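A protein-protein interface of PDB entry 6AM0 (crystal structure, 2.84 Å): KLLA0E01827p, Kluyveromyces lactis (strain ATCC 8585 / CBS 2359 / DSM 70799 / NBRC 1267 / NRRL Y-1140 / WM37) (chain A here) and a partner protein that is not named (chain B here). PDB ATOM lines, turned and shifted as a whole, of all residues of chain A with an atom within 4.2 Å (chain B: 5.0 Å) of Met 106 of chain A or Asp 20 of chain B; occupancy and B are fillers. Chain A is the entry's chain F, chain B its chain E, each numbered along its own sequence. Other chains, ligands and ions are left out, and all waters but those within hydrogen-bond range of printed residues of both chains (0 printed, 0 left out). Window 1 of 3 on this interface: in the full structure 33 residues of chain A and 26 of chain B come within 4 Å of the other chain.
The side-chain hydroxyl (OH) of Tyr 23 of chain A sits close to the side-chain carboxylate (OD2) of Asp 20 of chain B (2.4 Å). NH1 of Arg 24 of chain B lies within hydrogen-bond range of OD1 of Asn 113 of chain A. OH of Tyr 23 of chain A sits at hydrogen-bond distance from NH2 of Arg 24 of chain B, 2.7 Å away. The guanidinium group (NH1) of Arg 24 of chain B lies within hydrogen-bond range of the backbone carbonyl oxygen (O) of Asn 107 of chain A (2.5 Å).
The guanidinium group (NE) of Arg 24 of chain B is in salt-bridge range of the side-chain carboxylate (OD1) of Asp 20 of chain B (2.8 Å). The backbone NH (N) of Asn 107 of chain A lies within hydrogen-bond range of the side-chain amide oxygen (OD1) of Asn 113 of chain A. The side-chain amide nitrogen (ND2) of Asn 16 of chain B lies within hydrogen-bond range of the side-chain carboxylate (OE2) of Glu 19 of chain B, 3.1 Å away. The backbone carbonyl oxygen (O) of Gln 53 of chain A sits at hydrogen-bond distance from the backbone NH (N) of Arg 108 of chain A (2.6 Å). The backbone carbonyl oxygen of Val 55 of chain A is in hydrogen-bond range of the backbone NH of Met 106 of chain A (3.1 Å). The backbone carbonyl oxygen (O) of Ile 105 of chain A lies close to the side-chain amide oxygen (OD1) of Asn 113 of chain A (3.4 Å).
Among the printed residues, merely in contact across the chains: Arg 108 of chain A with Arg 24 of chain B, Tyr 23 of chain A with Phe 9 of chain B, Tyr 23 of chain A with Pro 8 of chain B, Val 19 of chain A with Val 23 of chain B, Met 106 of chain A with Asp 20 of chain B, Val 19 of chain A with Glu 19 of chain B, Val 19 of chain A with Asp 20 of chain B and Val 55 of chain A with Val 23 of chain B.
Of chain B, only Asp 20 comes within 4 Å of Met 106 of chain A. Asp 20 of chain B touches three residues of chain A. Of the printed residues of chain A, Glu 19 of chain B touches Val 19 (3.9 Å). Of the printed residues of chain A, Arg 24 of chain B touches Tyr 23 (2.7 Å), Asn 107 (2.5 Å), Arg 108 (3.4 Å) and Asn 113 (3.2 Å). Of the printed residues of chain A, Val 23 of chain B touches Val 19 and Val 55. The nearest printed residue of chain A that does not touch Asp 20 of chain B is Asn 113 of chain A (5.7 Å). The nearest printed residue of chain B that does not touch Val 19 of chain A is Asn 16 of chain B (5.3 Å).
Hydrophobic or aromatic side chains of chain A within 4 Å of the printed part of chain B: Val 19, Tyr 23, Val 55 and Met 106. Among the printed residues, 12 pairs touch across the chains. Among the printed residues, no Asp or Glu carboxylate lies within 4 Å of a Lys or Arg side-chain nitrogen of the other chain.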
ATOM      1  N   VAL A  19      18.984  20.091  -9.522  1.00  0.00           N
ATOM      2  CA  VAL A  19      17.785  19.627 -10.208  1.00  0.00           C
ATOM      3  C   VAL A  19      18.022  19.518 -11.708  1.00  0.00           C
ATOM      4  O   VAL A  19      17.749  18.476 -12.317  1.00  0.00           O
ATOM      5  CB  VAL A  19      16.600  20.554  -9.888  1.00  0.00           C
ATOM      6  CG1 VAL A  19      15.458  20.304 -10.864  1.00  0.00           C
ATOM      7  CG2 VAL A  19      16.146  20.333  -8.451  1.00  0.00           C
ATOM      8  N   TYR A  23      18.169  16.262 -15.226  1.00  0.00           N
ATOM      9  CA  TYR A  23      17.637  16.282 -16.582  1.00  0.00           C
ATOM     10  C   TYR A  23      18.749  16.299 -17.622  1.00  0.00           C
ATOM     11  O   TYR A  23      18.679  15.572 -18.618  1.00  0.00           O
ATOM     12  CB  TYR A  23      16.728  17.497 -16.779  1.00  0.00           C
ATOM     13  CG  TYR A  23      15.424  17.415 -16.021  1.00  0.00           C
ATOM     14  CD1 TYR A  23      15.327  17.884 -14.720  1.00  0.00           C
ATOM     15  CD2 TYR A  23      14.292  16.867 -16.608  1.00  0.00           C
ATOM     16  CE1 TYR A  23      14.139  17.810 -14.023  1.00  0.00           C
ATOM     17  CE2 TYR A  23      13.100  16.789 -15.918  1.00  0.00           C
ATOM     18  CZ  TYR A  23      13.030  17.263 -14.626  1.00  0.00           C
ATOM     19  OH  TYR A  23      11.845  17.190 -13.930  1.00  0.00           O
ATOM     20  N   GLN A  53       6.453  27.143 -19.539  1.00  0.00           N
ATOM     21  CA  GLN A  53       6.394  28.328 -18.692  1.00  0.00           C
ATOM     22  C   GLN A  53       7.091  28.083 -17.359  1.00  0.00           C
ATOM     23  O   GLN A  53       6.773  27.115 -16.658  1.00  0.00           O
ATOM     24  CB  GLN A  53       4.940  28.728 -18.449  1.00  0.00           C
ATOM     25  CG  GLN A  53       4.711  30.216 -18.427  1.00  0.00           C
ATOM     26  CD  GLN A  53       3.287  30.566 -18.078  1.00  0.00           C
ATOM     27  OE1 GLN A  53       2.524  29.712 -17.625  1.00  0.00           O
ATOM     28  NE2 GLN A  53       2.915  31.824 -18.287  1.00  0.00           N
ATOM     29  N   GLY A  54       8.024  28.950 -16.991  1.00  0.00           N
ATOM     30  CA  GLY A  54       8.718  28.801 -15.730  1.00  0.00           C
ATOM     31  C   GLY A  54      10.054  29.519 -15.749  1.00  0.00           C
ATOM     32  O   GLY A  54      10.345  30.320 -16.638  1.00  0.00           O
ATOM     33  N   VAL A  55      10.857  29.212 -14.727  1.00  0.00           N
ATOM     34  CA  VAL A  55      12.170  29.826 -14.597  1.00  0.00           C
ATOM     35  C   VAL A  55      13.057  29.390 -15.750  1.00  0.00           C
ATOM     36  O   VAL A  55      13.038  28.226 -16.172  1.00  0.00           O
ATOM     37  CB  VAL A  55      12.793  29.458 -13.240  1.00  0.00           C
ATOM     38  CG1 VAL A  55      12.696  27.958 -13.005  1.00  0.00           C
ATOM     39  CG2 VAL A  55      14.236  29.921 -13.168  1.00  0.00           C
ATOM     40  N   ILE A 104      17.348  26.097 -20.623  1.00  0.00           N
ATOM     41  CA  ILE A 104      16.269  25.264 -20.113  1.00  0.00           C
ATOM     42  C   ILE A 104      15.222  26.146 -19.447  1.00  0.00           C
ATOM     43  O   ILE A 104      15.540  27.170 -18.834  1.00  0.00           O
ATOM     44  CB  ILE A 104      16.794  24.183 -19.143  1.00  0.00           C
ATOM     45  CG1 ILE A 104      15.754  23.072 -18.973  1.00  0.00           C
ATOM     46  CG2 ILE A 104      17.171  24.785 -17.791  1.00  0.00           C
ATOM     47  CD1 ILE A 104      16.258  21.863 -18.215  1.00  0.00           C
ATOM     48  N   ILE A 105      13.963  25.757 -19.610  1.00  0.00           N
ATOM     49  CA  ILE A 105      12.843  26.340 -18.893  1.00  0.00           C
ATOM     50  C   ILE A 105      12.208  25.208 -18.107  1.00  0.00           C
ATOM     51  O   ILE A 105      11.665  24.259 -18.696  1.00  0.00           O
ATOM     52  CB  ILE A 105      11.825  27.000 -19.830  1.00  0.00           C
ATOM     53  CG1 ILE A 105      12.501  28.097 -20.646  1.00  0.00           C
ATOM     54  CG2 ILE A 105      10.650  27.555 -19.027  1.00  0.00           C
ATOM     55  CD1 ILE A 105      11.554  29.124 -21.177  1.00  0.00           C
ATOM     56  N   MET A 106      12.314  25.289 -16.784  1.00  0.00           N
ATOM     57  CA  MET A 106      11.641  24.354 -15.897  1.00  0.00           C
ATOM     58  C   MET A 106      10.144  24.607 -15.984  1.00  0.00           C
ATOM     59  O   MET A 106       9.647  25.629 -15.500  1.00  0.00           O
ATOM     60  CB  MET A 106      12.158  24.515 -14.472  1.00  0.00           C
ATOM     61  CG  MET A 106      13.651  24.272 -14.349  1.00  0.00           C
ATOM     62  SD  MET A 106      14.141  22.658 -14.997  1.00  0.00           S
ATOM     63  CE  MET A 106      13.299  21.562 -13.854  1.00  0.00           C
ATOM     64  N   ASN A 107       9.428  23.685 -16.613  1.00  0.00           N
ATOM     65  CA  ASN A 107       8.043  23.924 -16.980  1.00  0.00           C
ATOM     66  C   ASN A 107       7.130  23.785 -15.768  1.00  0.00           C
ATOM     67  O   ASN A 107       7.200  22.794 -15.034  1.00  0.00           O
ATOM     68  CB  ASN A 107       7.618  22.955 -18.080  1.00  0.00           C
ATOM     69  CG  ASN A 107       6.320  23.361 -18.740  1.00  0.00           C
ATOM     70  OD1 ASN A 107       5.826  24.471 -18.531  1.00  0.00           O
ATOM     71  ND2 ASN A 107       5.763  22.468 -19.548  1.00  0.00           N
ATOM     72  N   ARG A 108       6.281  24.794 -15.560  1.00  0.00           N
ATOM     73  CA  ARG A 108       5.216  24.735 -14.569  1.00  0.00           C
ATOM     74  C   ARG A 108       3.951  24.084 -15.106  1.00  0.00           C
ATOM     75  O   ARG A 108       3.120  23.624 -14.315  1.00  0.00           O
ATOM     76  CB  ARG A 108       4.863  26.143 -14.078  1.00  0.00           C
ATOM     77  CG  ARG A 108       6.008  26.929 -13.480  1.00  0.00           C
ATOM     78  CD  ARG A 108       5.541  28.320 -13.093  1.00  0.00           C
ATOM     79  NE  ARG A 108       4.404  28.267 -12.178  1.00  0.00           N
ATOM     80  CZ  ARG A 108       4.459  28.603 -10.893  1.00  0.00           C
ATOM     81  NH1 ARG A 108       5.598  29.029 -10.361  1.00  0.00           N
ATOM     82  NH2 ARG A 108       3.371  28.520 -10.139  1.00  0.00           N
ATOM     83  N   ASN A 113      10.309  19.841 -19.875  1.00  0.00           N
ATOM     84  CA  ASN A 113      10.986  21.126 -19.814  1.00  0.00           C
ATOM     85  C   ASN A 113      11.410  21.576 -21.202  1.00  0.00           C
ATOM     86  O   ASN A 113      11.628  20.760 -22.102  1.00  0.00           O
ATOM     87  CB  ASN A 113      12.206  21.048 -18.899  1.00  0.00           C
ATOM     88  CG  ASN A 113      11.833  20.760 -17.466  1.00  0.00           C
ATOM     89  OD1 ASN A 113      10.953  21.406 -16.900  1.00  0.00           O
ATOM     90  ND2 ASN A 113      12.491  19.773 -16.871  1.00  0.00           N
ATOM     91  N   PRO B   8      13.696  12.278 -14.626  1.00  0.00           N
ATOM     92  CA  PRO B   8      14.056  11.817 -13.276  1.00  0.00           C
ATOM     93  C   PRO B   8      12.857  11.369 -12.463  1.00  0.00           C
ATOM     94  O   PRO B   8      12.968  10.411 -11.690  1.00  0.00           O
ATOM     95  CB  PRO B   8      14.748  13.042 -12.661  1.00  0.00           C
ATOM     96  CG  PRO B   8      14.264  14.203 -13.456  1.00  0.00           C
ATOM     97  CD  PRO B   8      14.065  13.685 -14.848  1.00  0.00           C
ATOM     98  N   PHE B   9      11.703  12.011 -12.647  1.00  0.00           N
ATOM     99  CA  PHE B   9      10.488  11.685 -11.908  1.00  0.00           C
ATOM    100  C   PHE B   9      10.167  10.192 -11.921  1.00  0.00           C
ATOM    101  O   PHE B   9       9.489   9.695 -11.015  1.00  0.00           O
ATOM    102  CB  PHE B   9       9.304  12.468 -12.476  1.00  0.00           C
ATOM    103  CG  PHE B   9       9.213  13.885 -11.986  1.00  0.00           C
ATOM    104  CD1 PHE B   9       9.300  14.176 -10.637  1.00  0.00           C
ATOM    105  CD2 PHE B   9       9.027  14.926 -12.881  1.00  0.00           C
ATOM    106  CE1 PHE B   9       9.209  15.483 -10.189  1.00  0.00           C
ATOM    107  CE2 PHE B   9       8.935  16.233 -12.440  1.00  0.00           C
ATOM    108  CZ  PHE B   9       9.026  16.512 -11.094  1.00  0.00           C
ATOM    109  N   ASN B  16      13.910  14.167  -3.580  1.00  0.00           N
ATOM    110  CA  ASN B  16      14.446  14.866  -4.743  1.00  0.00           C
ATOM    111  C   ASN B  16      13.334  15.290  -5.697  1.00  0.00           C
ATOM    112  O   ASN B  16      13.435  16.336  -6.348  1.00  0.00           O
ATOM    113  CB  ASN B  16      15.478  13.993  -5.456  1.00  0.00           C
ATOM    114  CG  ASN B  16      16.584  13.517  -4.534  1.00  0.00           C
ATOM    115  OD1 ASN B  16      16.727  12.321  -4.289  1.00  0.00           O
ATOM    116  ND2 ASN B  16      17.380  14.451  -4.027  1.00  0.00           N
ATOM    117  N   ALA B  17      12.264  14.496  -5.794  1.00  0.00           N
ATOM    118  CA  ALA B  17      11.116  14.912  -6.594  1.00  0.00           C
ATOM    119  C   ALA B  17      10.483  16.172  -6.017  1.00  0.00           C
ATOM    120  O   ALA B  17      10.121  17.099  -6.757  1.00  0.00           O
ATOM    121  CB  ALA B  17      10.092  13.780  -6.678  1.00  0.00           C
ATOM    122  N   VAL B  18      10.359  16.231  -4.690  1.00  0.00           N
ATOM    123  CA  VAL B  18       9.949  17.470  -4.039  1.00  0.00           C
ATOM    124  C   VAL B  18      10.898  18.606  -4.409  1.00  0.00           C
ATOM    125  O   VAL B  18      10.462  19.729  -4.668  1.00  0.00           O
ATOM    126  CB  VAL B  18       9.864  17.279  -2.513  1.00  0.00           C
ATOM    127  CG1 VAL B  18       9.544  18.599  -1.835  1.00  0.00           C
ATOM    128  CG2 VAL B  18       8.809  16.244  -2.162  1.00  0.00           C
ATOM    129  N   GLU B  19      12.209  18.332  -4.448  1.00  0.00           N
ATOM    130  CA  GLU B  19      13.163  19.384  -4.805  1.00  0.00           C
ATOM    131  C   GLU B  19      12.892  19.914  -6.212  1.00  0.00           C
ATOM    132  O   GLU B  19      12.877  21.132  -6.441  1.00  0.00           O
ATOM    133  CB  GLU B  19      14.602  18.865  -4.688  1.00  0.00           C
ATOM    134  CG  GLU B  19      15.047  18.485  -3.269  1.00  0.00           C
ATOM    135  CD  GLU B  19      16.415  17.799  -3.226  1.00  0.00           C
ATOM    136  OE1 GLU B  19      16.908  17.517  -2.111  1.00  0.00           O
ATOM    137  OE2 GLU B  19      16.998  17.541  -4.301  1.00  0.00           O
ATOM    138  N   ASP B  20      12.671  19.004  -7.166  1.00  0.00           N
ATOM    139  CA  ASP B  20      12.277  19.381  -8.522  1.00  0.00           C
ATOM    140  C   ASP B  20      11.056  20.293  -8.505  1.00  0.00           C
ATOM    141  O   ASP B  20      11.069  21.387  -9.086  1.00  0.00           O
ATOM    142  CB  ASP B  20      11.997  18.113  -9.335  1.00  0.00           C
ATOM    143  CG  ASP B  20      11.930  18.364 -10.834  1.00  0.00           C
ATOM    144  OD1 ASP B  20      11.551  19.480 -11.255  1.00  0.00           O
ATOM    145  OD2 ASP B  20      12.255  17.426 -11.596  1.00  0.00           O
ATOM    146  N   LEU B  21       9.987  19.857  -7.832  1.00  0.00           N
ATOM    147  CA  LEU B  21       8.784  20.680  -7.738  1.00  0.00           C
ATOM    148  C   LEU B  21       9.083  22.052  -7.133  1.00  0.00           C
ATOM    149  O   LEU B  21       8.542  23.069  -7.585  1.00  0.00           O
ATOM    150  CB  LEU B  21       7.715  19.947  -6.925  1.00  0.00           C
ATOM    151  CG  LEU B  21       7.023  18.774  -7.631  1.00  0.00           C
ATOM    152  CD1 LEU B  21       6.234  17.919  -6.654  1.00  0.00           C
ATOM    153  CD2 LEU B  21       6.114  19.298  -8.719  1.00  0.00           C
ATOM    154  N   VAL B  22       9.955  22.105  -6.123  1.00  0.00           N
ATOM    155  CA  VAL B  22      10.255  23.374  -5.467  1.00  0.00           C
ATOM    156  C   VAL B  22      10.978  24.310  -6.426  1.00  0.00           C
ATOM    157  O   VAL B  22      10.741  25.525  -6.426  1.00  0.00           O
ATOM    158  CB  VAL B  22      11.061  23.142  -4.174  1.00  0.00           C
ATOM    159  CG1 VAL B  22      11.543  24.468  -3.595  1.00  0.00           C
ATOM    160  CG2 VAL B  22      10.216  22.409  -3.146  1.00  0.00           C
ATOM    161  N   VAL B  23      11.859  23.765  -7.267  1.00  0.00           N
ATOM    162  CA  VAL B  23      12.492  24.589  -8.295  1.00  0.00           C
ATOM    163  C   VAL B  23      11.448  25.092  -9.283  1.00  0.00           C
ATOM    164  O   VAL B  23      11.447  26.266  -9.671  1.00  0.00           O
ATOM    165  CB  VAL B  23      13.611  23.806  -9.004  1.00  0.00           C
ATOM    166  CG1 VAL B  23      14.059  24.541 -10.254  1.00  0.00           C
ATOM    167  CG2 VAL B  23      14.783  23.608  -8.064  1.00  0.00           C
ATOM    168  N   ARG B  24      10.526  24.213  -9.685  1.00  0.00           N
ATOM    169  CA  ARG B  24       9.563  24.573 -10.721  1.00  0.00           C
ATOM    170  C   ARG B  24       8.600  25.660 -10.254  1.00  0.00           C
ATOM    171  O   ARG B  24       8.266  26.572 -11.020  1.00  0.00           O
ATOM    172  CB  ARG B  24       8.773  23.340 -11.159  1.00  0.00           C
ATOM    173  CG  ARG B  24       9.564  22.320 -11.953  1.00  0.00           C
ATOM    174  CD  ARG B  24       8.729  21.072 -12.173  1.00  0.00           C
ATOM    175  NE  ARG B  24       9.433  20.060 -12.950  1.00  0.00           N
ATOM    176  CZ  ARG B  24       9.295  19.902 -14.261  1.00  0.00           C
ATOM    177  NH1 ARG B  24       8.478  20.694 -14.940  1.00  0.00           N
ATOM    178  NH2 ARG B  24       9.972  18.952 -14.892  1.00  0.00           N
